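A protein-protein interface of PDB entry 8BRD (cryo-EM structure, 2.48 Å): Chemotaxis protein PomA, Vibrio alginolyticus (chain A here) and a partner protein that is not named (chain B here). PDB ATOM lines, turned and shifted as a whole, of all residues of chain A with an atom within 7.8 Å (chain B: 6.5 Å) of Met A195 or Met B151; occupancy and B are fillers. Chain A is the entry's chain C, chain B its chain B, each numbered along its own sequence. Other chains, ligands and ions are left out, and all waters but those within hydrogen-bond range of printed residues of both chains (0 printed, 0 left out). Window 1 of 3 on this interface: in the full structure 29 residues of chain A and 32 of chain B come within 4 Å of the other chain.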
ATOM      1  N   LEU A   7      17.610   2.748 -18.528  1.00  0.00           N
ATOM      2  CA  LEU A   7      16.771   2.528 -17.359  1.00  0.00           C
ATOM      3  C   LEU A   7      17.621   2.547 -16.099  1.00  0.00           C
ATOM      4  O   LEU A   7      17.208   3.105 -15.085  1.00  0.00           O
ATOM      5  CB  LEU A   7      16.012   1.204 -17.481  1.00  0.00           C
ATOM      6  CG  LEU A   7      15.613   0.475 -16.197  1.00  0.00           C
ATOM      7  CD1 LEU A   7      14.434   1.151 -15.515  1.00  0.00           C
ATOM      8  CD2 LEU A   7      15.293  -0.972 -16.509  1.00  0.00           C
ATOM      9  N   GLY A   8      18.813   1.954 -16.162  1.00  0.00           N
ATOM     10  CA  GLY A   8      19.691   1.953 -15.004  1.00  0.00           C
ATOM     11  C   GLY A   8      20.175   3.338 -14.627  1.00  0.00           C
ATOM     12  O   GLY A   8      20.253   3.679 -13.448  1.00  0.00           O
ATOM     13  N   GLY A  11      17.236   5.184 -13.188  1.00  0.00           N
ATOM     14  CA  GLY A  11      16.959   4.607 -11.885  1.00  0.00           C
ATOM     15  C   GLY A  11      17.959   5.037 -10.833  1.00  0.00           C
ATOM     16  O   GLY A  11      17.586   5.321  -9.698  1.00  0.00           O
ATOM     17  N   GLY A  12      19.240   5.097 -11.196  1.00  0.00           N
ATOM     18  CA  GLY A  12      20.245   5.572 -10.262  1.00  0.00           C
ATOM     19  C   GLY A  12      20.088   7.044  -9.931  1.00  0.00           C
ATOM     20  O   GLY A  12      20.292   7.458  -8.789  1.00  0.00           O
ATOM     21  N   PHE A  15      17.222   7.248  -7.682  1.00  0.00           N
ATOM     22  CA  PHE A  15      17.630   6.683  -6.404  1.00  0.00           C
ATOM     23  C   PHE A  15      18.430   7.686  -5.586  1.00  0.00           C
ATOM     24  O   PHE A  15      18.252   7.791  -4.370  1.00  0.00           O
ATOM     25  CB  PHE A  15      18.439   5.412  -6.641  1.00  0.00           C
ATOM     26  CG  PHE A  15      19.095   4.882  -5.411  1.00  0.00           C
ATOM     27  CD1 PHE A  15      18.356   4.242  -4.436  1.00  0.00           C
ATOM     28  CD2 PHE A  15      20.457   5.033  -5.224  1.00  0.00           C
ATOM     29  CE1 PHE A  15      18.965   3.760  -3.307  1.00  0.00           C
ATOM     30  CE2 PHE A  15      21.066   4.553  -4.093  1.00  0.00           C
ATOM     31  CZ  PHE A  15      20.323   3.916  -3.139  1.00  0.00           C
ATOM     32  N   PHE A  66      29.619  -0.510 -23.101  1.00  0.00           N
ATOM     33  CA  PHE A  66      28.623   0.460 -22.672  1.00  0.00           C
ATOM     34  C   PHE A  66      28.632   1.740 -23.500  1.00  0.00           C
ATOM     35  O   PHE A  66      27.784   2.607 -23.277  1.00  0.00           O
ATOM     36  CB  PHE A  66      28.818   0.800 -21.194  1.00  0.00           C
ATOM     37  CG  PHE A  66      28.260  -0.232 -20.258  1.00  0.00           C
ATOM     38  CD1 PHE A  66      28.900  -1.446 -20.083  1.00  0.00           C
ATOM     39  CD2 PHE A  66      27.088   0.007 -19.565  1.00  0.00           C
ATOM     40  CE1 PHE A  66      28.390  -2.396 -19.229  1.00  0.00           C
ATOM     41  CE2 PHE A  66      26.572  -0.941 -18.711  1.00  0.00           C
ATOM     42  CZ  PHE A  66      27.226  -2.144 -18.541  1.00  0.00           C
ATOM     43  N   TYR A 188      27.293   0.583   0.278  1.00  0.00           N
ATOM     44  CA  TYR A 188      28.173   0.679  -0.882  1.00  0.00           C
ATOM     45  C   TYR A 188      28.429  -0.689  -1.491  1.00  0.00           C
ATOM     46  O   TYR A 188      28.387  -0.846  -2.713  1.00  0.00           O
ATOM     47  CB  TYR A 188      29.507   1.318  -0.502  1.00  0.00           C
ATOM     48  CG  TYR A 188      29.430   2.779  -0.160  1.00  0.00           C
ATOM     49  CD1 TYR A 188      28.373   3.557  -0.596  1.00  0.00           C
ATOM     50  CD2 TYR A 188      30.428   3.381   0.584  1.00  0.00           C
ATOM     51  CE1 TYR A 188      28.306   4.887  -0.284  1.00  0.00           C
ATOM     52  CE2 TYR A 188      30.368   4.710   0.897  1.00  0.00           C
ATOM     53  CZ  TYR A 188      29.310   5.459   0.461  1.00  0.00           C
ATOM     54  OH  TYR A 188      29.252   6.790   0.774  1.00  0.00           O
ATOM     55  N   GLY A 189      28.714  -1.685  -0.653  1.00  0.00           N
ATOM     56  CA  GLY A 189      28.948  -3.023  -1.168  1.00  0.00           C
ATOM     57  C   GLY A 189      27.744  -3.583  -1.894  1.00  0.00           C
ATOM     58  O   GLY A 189      27.873  -4.170  -2.970  1.00  0.00           O
ATOM     59  N   ALA A 190      26.549  -3.389  -1.325  1.00  0.00           N
ATOM     60  CA  ALA A 190      25.325  -3.881  -1.947  1.00  0.00           C
ATOM     61  C   ALA A 190      25.055  -3.191  -3.275  1.00  0.00           C
ATOM     62  O   ALA A 190      24.742  -3.857  -4.270  1.00  0.00           O
ATOM     63  CB  ALA A 190      24.143  -3.690  -0.999  1.00  0.00           C
ATOM     64  N   ILE A 191      25.171  -1.863  -3.320  1.00  0.00           N
ATOM     65  CA  ILE A 191      24.909  -1.145  -4.564  1.00  0.00           C
ATOM     66  C   ILE A 191      25.935  -1.522  -5.624  1.00  0.00           C
ATOM     67  O   ILE A 191      25.589  -1.781  -6.781  1.00  0.00           O
ATOM     68  CB  ILE A 191      24.876   0.373  -4.317  1.00  0.00           C
ATOM     69  CG1 ILE A 191      23.569   0.767  -3.637  1.00  0.00           C
ATOM     70  CG2 ILE A 191      25.029   1.130  -5.625  1.00  0.00           C
ATOM     71  CD1 ILE A 191      23.567   2.169  -3.116  1.00  0.00           C
ATOM     72  N   LEU A 192      27.214  -1.569  -5.247  1.00  0.00           N
ATOM     73  CA  LEU A 192      28.255  -1.889  -6.214  1.00  0.00           C
ATOM     74  C   LEU A 192      28.104  -3.308  -6.740  1.00  0.00           C
ATOM     75  O   LEU A 192      28.277  -3.553  -7.936  1.00  0.00           O
ATOM     76  CB  LEU A 192      29.631  -1.692  -5.583  1.00  0.00           C
ATOM     77  CG  LEU A 192      30.117  -0.253  -5.416  1.00  0.00           C
ATOM     78  CD1 LEU A 192      31.506  -0.242  -4.829  1.00  0.00           C
ATOM     79  CD2 LEU A 192      30.089   0.477  -6.743  1.00  0.00           C
ATOM     80  N   SER A 193      27.779  -4.256  -5.861  1.00  0.00           N
ATOM     81  CA  SER A 193      27.628  -5.641  -6.281  1.00  0.00           C
ATOM     82  C   SER A 193      26.396  -5.818  -7.159  1.00  0.00           C
ATOM     83  O   SER A 193      26.499  -6.218  -8.323  1.00  0.00           O
ATOM     84  CB  SER A 193      27.549  -6.537  -5.048  1.00  0.00           C
ATOM     85  OG  SER A 193      27.266  -7.874  -5.402  1.00  0.00           O
ATOM     86  N   ASN A 194      25.219  -5.516  -6.615  1.00  0.00           N
ATOM     87  CA  ASN A 194      23.977  -5.860  -7.293  1.00  0.00           C
ATOM     88  C   ASN A 194      23.657  -4.926  -8.447  1.00  0.00           C
ATOM     89  O   ASN A 194      23.026  -5.350  -9.419  1.00  0.00           O
ATOM     90  CB  ASN A 194      22.825  -5.865  -6.292  1.00  0.00           C
ATOM     91  CG  ASN A 194      22.971  -6.952  -5.253  1.00  0.00           C
ATOM     92  OD1 ASN A 194      22.931  -6.689  -4.053  1.00  0.00           O
ATOM     93  ND2 ASN A 194      23.152  -8.182  -5.710  1.00  0.00           N
ATOM     94  N   MET A 195      24.074  -3.666  -8.372  1.00  0.00           N
ATOM     95  CA  MET A 195      23.634  -2.667  -9.330  1.00  0.00           C
ATOM     96  C   MET A 195      24.720  -2.220 -10.295  1.00  0.00           C
ATOM     97  O   MET A 195      24.401  -1.544 -11.278  1.00  0.00           O
ATOM     98  CB  MET A 195      23.075  -1.441  -8.589  1.00  0.00           C
ATOM     99  CG  MET A 195      21.878  -1.750  -7.695  1.00  0.00           C
ATOM    100  SD  MET A 195      20.487  -2.518  -8.539  1.00  0.00           S
ATOM    101  CE  MET A 195      19.808  -1.113  -9.405  1.00  0.00           C
ATOM    102  N   VAL A 196      25.984  -2.569 -10.052  1.00  0.00           N
ATOM    103  CA  VAL A 196      27.064  -2.130 -10.933  1.00  0.00           C
ATOM    104  C   VAL A 196      27.863  -3.313 -11.473  1.00  0.00           C
ATOM    105  O   VAL A 196      27.864  -3.567 -12.678  1.00  0.00           O
ATOM    106  CB  VAL A 196      27.990  -1.131 -10.216  1.00  0.00           C
ATOM    107  CG1 VAL A 196      29.056  -0.624 -11.166  1.00  0.00           C
ATOM    108  CG2 VAL A 196      27.192   0.024  -9.647  1.00  0.00           C
ATOM    109  N   PHE A 197      28.537  -4.052 -10.587  1.00  0.00           N
ATOM    110  CA  PHE A 197      29.520  -5.036 -11.042  1.00  0.00           C
ATOM    111  C   PHE A 197      28.852  -6.246 -11.684  1.00  0.00           C
ATOM    112  O   PHE A 197      29.271  -6.703 -12.755  1.00  0.00           O
ATOM    113  CB  PHE A 197      30.412  -5.472  -9.879  1.00  0.00           C
ATOM    114  CG  PHE A 197      31.306  -4.389  -9.368  1.00  0.00           C
ATOM    115  CD1 PHE A 197      32.039  -3.612 -10.244  1.00  0.00           C
ATOM    116  CD2 PHE A 197      31.410  -4.141  -8.011  1.00  0.00           C
ATOM    117  CE1 PHE A 197      32.857  -2.606  -9.779  1.00  0.00           C
ATOM    118  CE2 PHE A 197      32.230  -3.138  -7.542  1.00  0.00           C
ATOM    119  CZ  PHE A 197      32.953  -2.369  -8.425  1.00  0.00           C
ATOM    120  N   PHE A 198      27.835  -6.795 -11.034  1.00  0.00           N
ATOM    121  CA  PHE A 198      27.090  -7.913 -11.601  1.00  0.00           C
ATOM    122  C   PHE A 198      26.345  -7.494 -12.865  1.00  0.00           C
ATOM    123  O   PHE A 198      26.326  -8.260 -13.834  1.00  0.00           O
ATOM    124  CB  PHE A 198      26.137  -8.514 -10.566  1.00  0.00           C
ATOM    125  CG  PHE A 198      26.824  -9.370  -9.544  1.00  0.00           C
ATOM    126  CD1 PHE A 198      27.949 -10.097  -9.880  1.00  0.00           C
ATOM    127  CD2 PHE A 198      26.345  -9.451  -8.251  1.00  0.00           C
ATOM    128  CE1 PHE A 198      28.583 -10.888  -8.948  1.00  0.00           C
ATOM    129  CE2 PHE A 198      26.978 -10.241  -7.314  1.00  0.00           C
ATOM    130  CZ  PHE A 198      28.097 -10.959  -7.664  1.00  0.00           C
ATOM    131  N   PRO A 199      25.689  -6.328 -12.903  1.00  0.00           N
ATOM    132  CA  PRO A 199      25.128  -5.873 -14.186  1.00  0.00           C
ATOM    133  C   PRO A 199      26.156  -5.716 -15.290  1.00  0.00           C
ATOM    134  O   PRO A 199      25.862  -6.055 -16.440  1.00  0.00           O
ATOM    135  CB  PRO A 199      24.483  -4.535 -13.815  1.00  0.00           C
ATOM    136  CG  PRO A 199      24.078  -4.722 -12.435  1.00  0.00           C
ATOM    137  CD  PRO A 199      25.184  -5.498 -11.796  1.00  0.00           C
ATOM    138  N   ILE A 200      27.354  -5.211 -14.984  1.00  0.00           N
ATOM    139  CA  ILE A 200      28.383  -5.090 -16.011  1.00  0.00           C
ATOM    140  C   ILE A 200      28.817  -6.467 -16.494  1.00  0.00           C
ATOM    141  O   ILE A 200      28.999  -6.685 -17.693  1.00  0.00           O
ATOM    142  CB  ILE A 200      29.579  -4.270 -15.495  1.00  0.00           C
ATOM    143  CG1 ILE A 200      29.212  -2.793 -15.390  1.00  0.00           C
ATOM    144  CG2 ILE A 200      30.764  -4.412 -16.422  1.00  0.00           C
ATOM    145  CD1 ILE A 200      30.311  -1.941 -14.813  1.00  0.00           C
ATOM    146  N   LEU B  34       9.250   1.545  -6.171  1.00  0.00           N
ATOM    147  CA  LEU B  34      10.234   1.908  -7.181  1.00  0.00           C
ATOM    148  C   LEU B  34      11.573   1.245  -6.900  1.00  0.00           C
ATOM    149  O   LEU B  34      12.120   0.560  -7.766  1.00  0.00           O
ATOM    150  CB  LEU B  34      10.377   3.428  -7.261  1.00  0.00           C
ATOM    151  CG  LEU B  34       9.218   4.163  -7.938  1.00  0.00           C
ATOM    152  CD1 LEU B  34       9.563   5.625  -8.166  1.00  0.00           C
ATOM    153  CD2 LEU B  34       8.841   3.488  -9.245  1.00  0.00           C
ATOM    154  N   ILE B  35      12.082   1.377  -5.672  1.00  0.00           N
ATOM    155  CA  ILE B  35      13.382   0.796  -5.339  1.00  0.00           C
ATOM    156  C   ILE B  35      13.403  -0.695  -5.639  1.00  0.00           C
ATOM    157  O   ILE B  35      14.350  -1.207  -6.247  1.00  0.00           O
ATOM    158  CB  ILE B  35      13.738   1.073  -3.867  1.00  0.00           C
ATOM    159  CG1 ILE B  35      13.936   2.568  -3.631  1.00  0.00           C
ATOM    160  CG2 ILE B  35      14.973   0.286  -3.463  1.00  0.00           C
ATOM    161  CD1 ILE B  35      14.020   2.943  -2.179  1.00  0.00           C
ATOM    162  N   VAL B  36      12.361  -1.415  -5.235  1.00  0.00           N
ATOM    163  CA  VAL B  36      12.377  -2.861  -5.418  1.00  0.00           C
ATOM    164  C   VAL B  36      12.098  -3.262  -6.865  1.00  0.00           C
ATOM    165  O   VAL B  36      12.926  -3.936  -7.486  1.00  0.00           O
ATOM    166  CB  VAL B  36      11.387  -3.535  -4.449  1.00  0.00           C
ATOM    167  CG1 VAL B  36      11.274  -5.023  -4.747  1.00  0.00           C
ATOM    168  CG2 VAL B  36      11.835  -3.324  -3.019  1.00  0.00           C
ATOM    169  N   VAL B  37      10.964  -2.839  -7.425  1.00  0.00           N
ATOM    170  CA  VAL B  37      10.557  -3.269  -8.755  1.00  0.00           C
ATOM    171  C   VAL B  37      11.507  -2.740  -9.823  1.00  0.00           C
ATOM    172  O   VAL B  37      11.938  -3.495 -10.699  1.00  0.00           O
ATOM    173  CB  VAL B  37       9.105  -2.834  -9.027  1.00  0.00           C
ATOM    174  CG1 VAL B  37       8.697  -3.188 -10.446  1.00  0.00           C
ATOM    175  CG2 VAL B  37       8.165  -3.469  -8.022  1.00  0.00           C
ATOM    176  N   GLY B  38      11.822  -1.441  -9.801  1.00  0.00           N
ATOM    177  CA  GLY B  38      12.683  -0.888 -10.831  1.00  0.00           C
ATOM    178  C   GLY B  38      14.093  -1.433 -10.767  1.00  0.00           C
ATOM    179  O   GLY B  38      14.711  -1.714 -11.796  1.00  0.00           O
ATOM    180  N   GLY B  39      14.627  -1.588  -9.556  1.00  0.00           N
ATOM    181  CA  GLY B  39      15.934  -2.202  -9.414  1.00  0.00           C
ATOM    182  C   GLY B  39      15.958  -3.632  -9.918  1.00  0.00           C
ATOM    183  O   GLY B  39      16.897  -4.043 -10.610  1.00  0.00           O
ATOM    184  N   SER B  40      14.921  -4.405  -9.591  1.00  0.00           N
ATOM    185  CA  SER B  40      14.836  -5.778 -10.075  1.00  0.00           C
ATOM    186  C   SER B  40      14.743  -5.818 -11.593  1.00  0.00           C
ATOM    187  O   SER B  40      15.398  -6.635 -12.245  1.00  0.00           O
ATOM    188  CB  SER B  40      13.632  -6.474  -9.442  1.00  0.00           C
ATOM    189  OG  SER B  40      13.516  -6.140  -8.075  1.00  0.00           O
ATOM    190  N   PHE B  42      15.794  -3.555 -13.734  1.00  0.00           N
ATOM    191  CA  PHE B  42      17.088  -3.181 -14.289  1.00  0.00           C
ATOM    192  C   PHE B  42      18.059  -4.353 -14.256  1.00  0.00           C
ATOM    193  O   PHE B  42      18.693  -4.673 -15.266  1.00  0.00           O
ATOM    194  CB  PHE B  42      17.657  -1.985 -13.527  1.00  0.00           C
ATOM    195  CG  PHE B  42      19.139  -1.829 -13.672  1.00  0.00           C
ATOM    196  CD1 PHE B  42      19.692  -1.395 -14.861  1.00  0.00           C
ATOM    197  CD2 PHE B  42      19.985  -2.130 -12.625  1.00  0.00           C
ATOM    198  CE1 PHE B  42      21.054  -1.251 -14.991  1.00  0.00           C
ATOM    199  CE2 PHE B  42      21.345  -1.991 -12.751  1.00  0.00           C
ATOM    200  CZ  PHE B  42      21.882  -1.553 -13.936  1.00  0.00           C
ATOM    201  N   VAL B  43      18.179  -5.016 -13.105  1.00  0.00           N
ATOM    202  CA  VAL B  43      19.121  -6.128 -12.987  1.00  0.00           C
ATOM    203  C   VAL B  43      18.759  -7.248 -13.956  1.00  0.00           C
ATOM    204  O   VAL B  43      19.629  -7.812 -14.635  1.00  0.00           O
ATOM    205  CB  VAL B  43      19.173  -6.624 -11.529  1.00  0.00           C
ATOM    206  CG1 VAL B  43      19.921  -7.934 -11.430  1.00  0.00           C
ATOM    207  CG2 VAL B  43      19.814  -5.574 -10.638  1.00  0.00           C
ATOM    208  N   ASP B 146      15.790 -13.619  -7.127  1.00  0.00           N
ATOM    209  CA  ASP B 146      17.080 -13.410  -6.484  1.00  0.00           C
ATOM    210  C   ASP B 146      17.347 -11.933  -6.245  1.00  0.00           C
ATOM    211  O   ASP B 146      17.894 -11.560  -5.203  1.00  0.00           O
ATOM    212  CB  ASP B 146      18.199 -14.011  -7.334  1.00  0.00           C
ATOM    213  CG  ASP B 146      18.211 -15.522  -7.296  1.00  0.00           C
ATOM    214  OD1 ASP B 146      17.951 -16.094  -6.218  1.00  0.00           O
ATOM    215  OD2 ASP B 146      18.484 -16.139  -8.347  1.00  0.00           O
ATOM    216  N   VAL B 147      16.969 -11.077  -7.195  1.00  0.00           N
ATOM    217  CA  VAL B 147      17.303  -9.666  -7.053  1.00  0.00           C
ATOM    218  C   VAL B 147      16.344  -8.951  -6.106  1.00  0.00           C
ATOM    219  O   VAL B 147      16.739  -7.990  -5.440  1.00  0.00           O
ATOM    220  CB  VAL B 147      17.359  -8.983  -8.432  1.00  0.00           C
ATOM    221  CG1 VAL B 147      16.021  -9.039  -9.117  1.00  0.00           C
ATOM    222  CG2 VAL B 147      17.818  -7.545  -8.298  1.00  0.00           C
ATOM    223  N   ALA B 148      15.086  -9.398  -6.014  1.00  0.00           N
ATOM    224  CA  ALA B 148      14.120  -8.690  -5.175  1.00  0.00           C
ATOM    225  C   ALA B 148      14.558  -8.565  -3.719  1.00  0.00           C
ATOM    226  O   ALA B 148      14.464  -7.455  -3.166  1.00  0.00           O
ATOM    227  CB  ALA B 148      12.746  -9.358  -5.301  1.00  0.00           C
ATOM    228  N   PRO B 149      15.025  -9.620  -3.038  1.00  0.00           N
ATOM    229  CA  PRO B 149      15.539  -9.414  -1.675  1.00  0.00           C
ATOM    230  C   PRO B 149      16.780  -8.538  -1.616  1.00  0.00           C
ATOM    231  O   PRO B 149      16.963  -7.817  -0.631  1.00  0.00           O
ATOM    232  CB  PRO B 149      15.831 -10.843  -1.191  1.00  0.00           C
ATOM    233  CG  PRO B 149      15.059 -11.718  -2.092  1.00  0.00           C
ATOM    234  CD  PRO B 149      15.068 -11.044  -3.406  1.00  0.00           C
ATOM    235  N   ALA B 150      17.645  -8.584  -2.632  1.00  0.00           N
ATOM    236  CA  ALA B 150      18.795  -7.686  -2.670  1.00  0.00           C
ATOM    237  C   ALA B 150      18.353  -6.229  -2.746  1.00  0.00           C
ATOM    238  O   ALA B 150      18.922  -5.361  -2.075  1.00  0.00           O
ATOM    239  CB  ALA B 150      19.694  -8.039  -3.851  1.00  0.00           C
ATOM    240  N   MET B 151      17.330  -5.944  -3.552  1.00  0.00           N
ATOM    241  CA  MET B 151      16.772  -4.598  -3.582  1.00  0.00           C
ATOM    242  C   MET B 151      16.116  -4.236  -2.261  1.00  0.00           C
ATOM    243  O   MET B 151      16.195  -3.080  -1.830  1.00  0.00           O
ATOM    244  CB  MET B 151      15.764  -4.468  -4.725  1.00  0.00           C
ATOM    245  CG  MET B 151      16.342  -4.709  -6.107  1.00  0.00           C
ATOM    246  SD  MET B 151      17.960  -3.976  -6.398  1.00  0.00           S
ATOM    247  CE  MET B 151      17.632  -2.251  -6.063  1.00  0.00           C
ATOM    248  N   GLY B 152      15.459  -5.198  -1.611  1.00  0.00           N
ATOM    249  CA  GLY B 152      14.914  -4.941  -0.289  1.00  0.00           C
ATOM    250  C   GLY B 152      15.981  -4.567   0.717  1.00  0.00           C
ATOM    251  O   GLY B 152      15.788  -3.668   1.533  1.00  0.00           O
ATOM    252  N   MET B 153      17.129  -5.244   0.662  1.00  0.00           N
ATOM    253  CA  MET B 153      18.238  -4.917   1.554  1.00  0.00           C
ATOM    254  C   MET B 153      18.853  -3.564   1.225  1.00  0.00           C
ATOM    255  O   MET B 153      19.218  -2.819   2.139  1.00  0.00           O
ATOM    256  CB  MET B 153      19.300  -6.013   1.497  1.00  0.00           C
ATOM    257  CG  MET B 153      20.529  -5.734   2.349  1.00  0.00           C
ATOM    258  SD  MET B 153      20.554  -6.666   3.890  1.00  0.00           S
ATOM    259  CE  MET B 153      20.362  -5.351   5.088  1.00  0.00           C
ATOM    260  N   ILE B 154      18.977  -3.229  -0.060  1.00  0.00           N
ATOM    261  CA  ILE B 154      19.453  -1.902  -0.444  1.00  0.00           C
ATOM    262  C   ILE B 154      18.518  -0.827   0.102  1.00  0.00           C
ATOM    263  O   ILE B 154      18.961   0.196   0.639  1.00  0.00           O
ATOM    264  CB  ILE B 154      19.595  -1.803  -1.973  1.00  0.00           C
ATOM    265  CG1 ILE B 154      20.866  -2.512  -2.440  1.00  0.00           C
ATOM    266  CG2 ILE B 154      19.591  -0.346  -2.424  1.00  0.00           C
ATOM    267  CD1 ILE B 154      20.997  -2.611  -3.936  1.00  0.00           C
ATOM    268  N   GLY B 155      17.208  -1.045  -0.032  1.00  0.00           N
ATOM    269  CA  GLY B 155      16.249  -0.091   0.501  1.00  0.00           C
ATOM    270  C   GLY B 155      16.297   0.005   2.011  1.00  0.00           C
ATOM    271  O   GLY B 155      16.150   1.088   2.578  1.00  0.00           O
ATOM    272  N   THR B 156      16.512  -1.126   2.680  1.00  0.00           N
ATOM    273  CA  THR B 156      16.669  -1.119   4.129  1.00  0.00           C
ATOM    274  C   THR B 156      17.891  -0.315   4.544  1.00  0.00           C
ATOM    275  O   THR B 156      17.824   0.495   5.469  1.00  0.00           O
ATOM    276  CB  THR B 156      16.770  -2.551   4.646  1.00  0.00           C
ATOM    277  OG1 THR B 156      15.469  -3.145   4.676  1.00  0.00           O
ATOM    278  CG2 THR B 156      17.367  -2.591   6.043  1.00  0.00           C
ATOM    279  N   THR B 183      10.448  -1.928   1.679  1.00  0.00           N
ATOM    280  CA  THR B 183      11.305  -2.516   0.656  1.00  0.00           C
ATOM    281  C   THR B 183      11.587  -3.981   0.958  1.00  0.00           C
ATOM    282  O   THR B 183      11.524  -4.834   0.070  1.00  0.00           O
ATOM    283  CB  THR B 183      12.608  -1.728   0.552  1.00  0.00           C
ATOM    284  OG1 THR B 183      13.045  -1.367   1.865  1.00  0.00           O
ATOM    285  CG2 THR B 183      12.419  -0.479  -0.278  1.00  0.00           C
ATOM    286  N   THR B 184      11.900  -4.289   2.218  1.00  0.00           N
ATOM    287  CA  THR B 184      12.155  -5.668   2.615  1.00  0.00           C
ATOM    288  C   THR B 184      10.896  -6.515   2.518  1.00  0.00           C
ATOM    289  O   THR B 184      10.953  -7.648   2.029  1.00  0.00           O
ATOM    290  CB  THR B 184      12.719  -5.711   4.036  1.00  0.00           C
ATOM    291  OG1 THR B 184      14.038  -5.162   4.034  1.00  0.00           O
ATOM    292  CG2 THR B 184      12.797  -7.137   4.546  1.00  0.00           C
ATOM    293  N   GLY B 187      10.267  -7.084  -1.230  1.00  0.00           N
ATOM    294  CA  GLY B 187      11.236  -8.019  -1.771  1.00  0.00           C
ATOM    295  C   GLY B 187      10.954  -9.444  -1.343  1.00  0.00           C
ATOM    296  O   GLY B 187      11.004 -10.368  -2.155  1.00  0.00           O
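OD1 of Asn A194 lies close to O of Ala A190 (3.4 Å).
Among the printed residues, pairs that only touch across the chains: Leu A7 with Phe B42 (3.6 Å), Gly A8 with Phe B42 (3.4 Å), Ala A190 with Ile B154 (3.8 Å), Asn A194 with Val B43 (3.4 Å), Asn A194 with Ala B150 (3.5 Å), Met A195 with Phe B42 (3.4 Å), Met A195 with Val B43 (3.8 Å), Met A195 with Ile B154 (3.96 Å) and Pro A199 with Phe B42 (3.9 Å).
Of the printed residues of chain B, Gly A8 touches Phe B42.
Phe A15 touches none of the printed residues of chain B.
Of the printed residues of chain B, Ala A190 touches Ile B154.
Of the printed residues of chain B, Pro A199 touches Phe B42.
Val B36 touches none of the printed residues of chain A.
Of the printed residues of chain A, Phe B42 touches Leu A7 (3.6 Å), Gly A8 (3.4 Å), Met A195 (3.4 Å) and Pro A199 (3.9 Å).
Printed residues of chain A within 4 Å of Met B151: Met A195.
Gly B152 touches none of the printed residues of chain A.
Of the printed residues of chain A, Ile B154 touches Ala A190 and Met A195.
Of the 23 printed residues of chain B, 5 touch a printed residue of chain A.
Of the 19 printed residues of chain A, 6 touch a printed residue of chain B.
Among the printed residues, 10 pairs touch across the chains.
Among the printed residues, no Asp or Glu carboxylate lies within 4 Å of a Lys or Arg side-chain nitrogen of the other chain.
The side-chain sulfur of Met B151 lies close to the side-chain sulfur of Met A195, at 3.6 Å.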
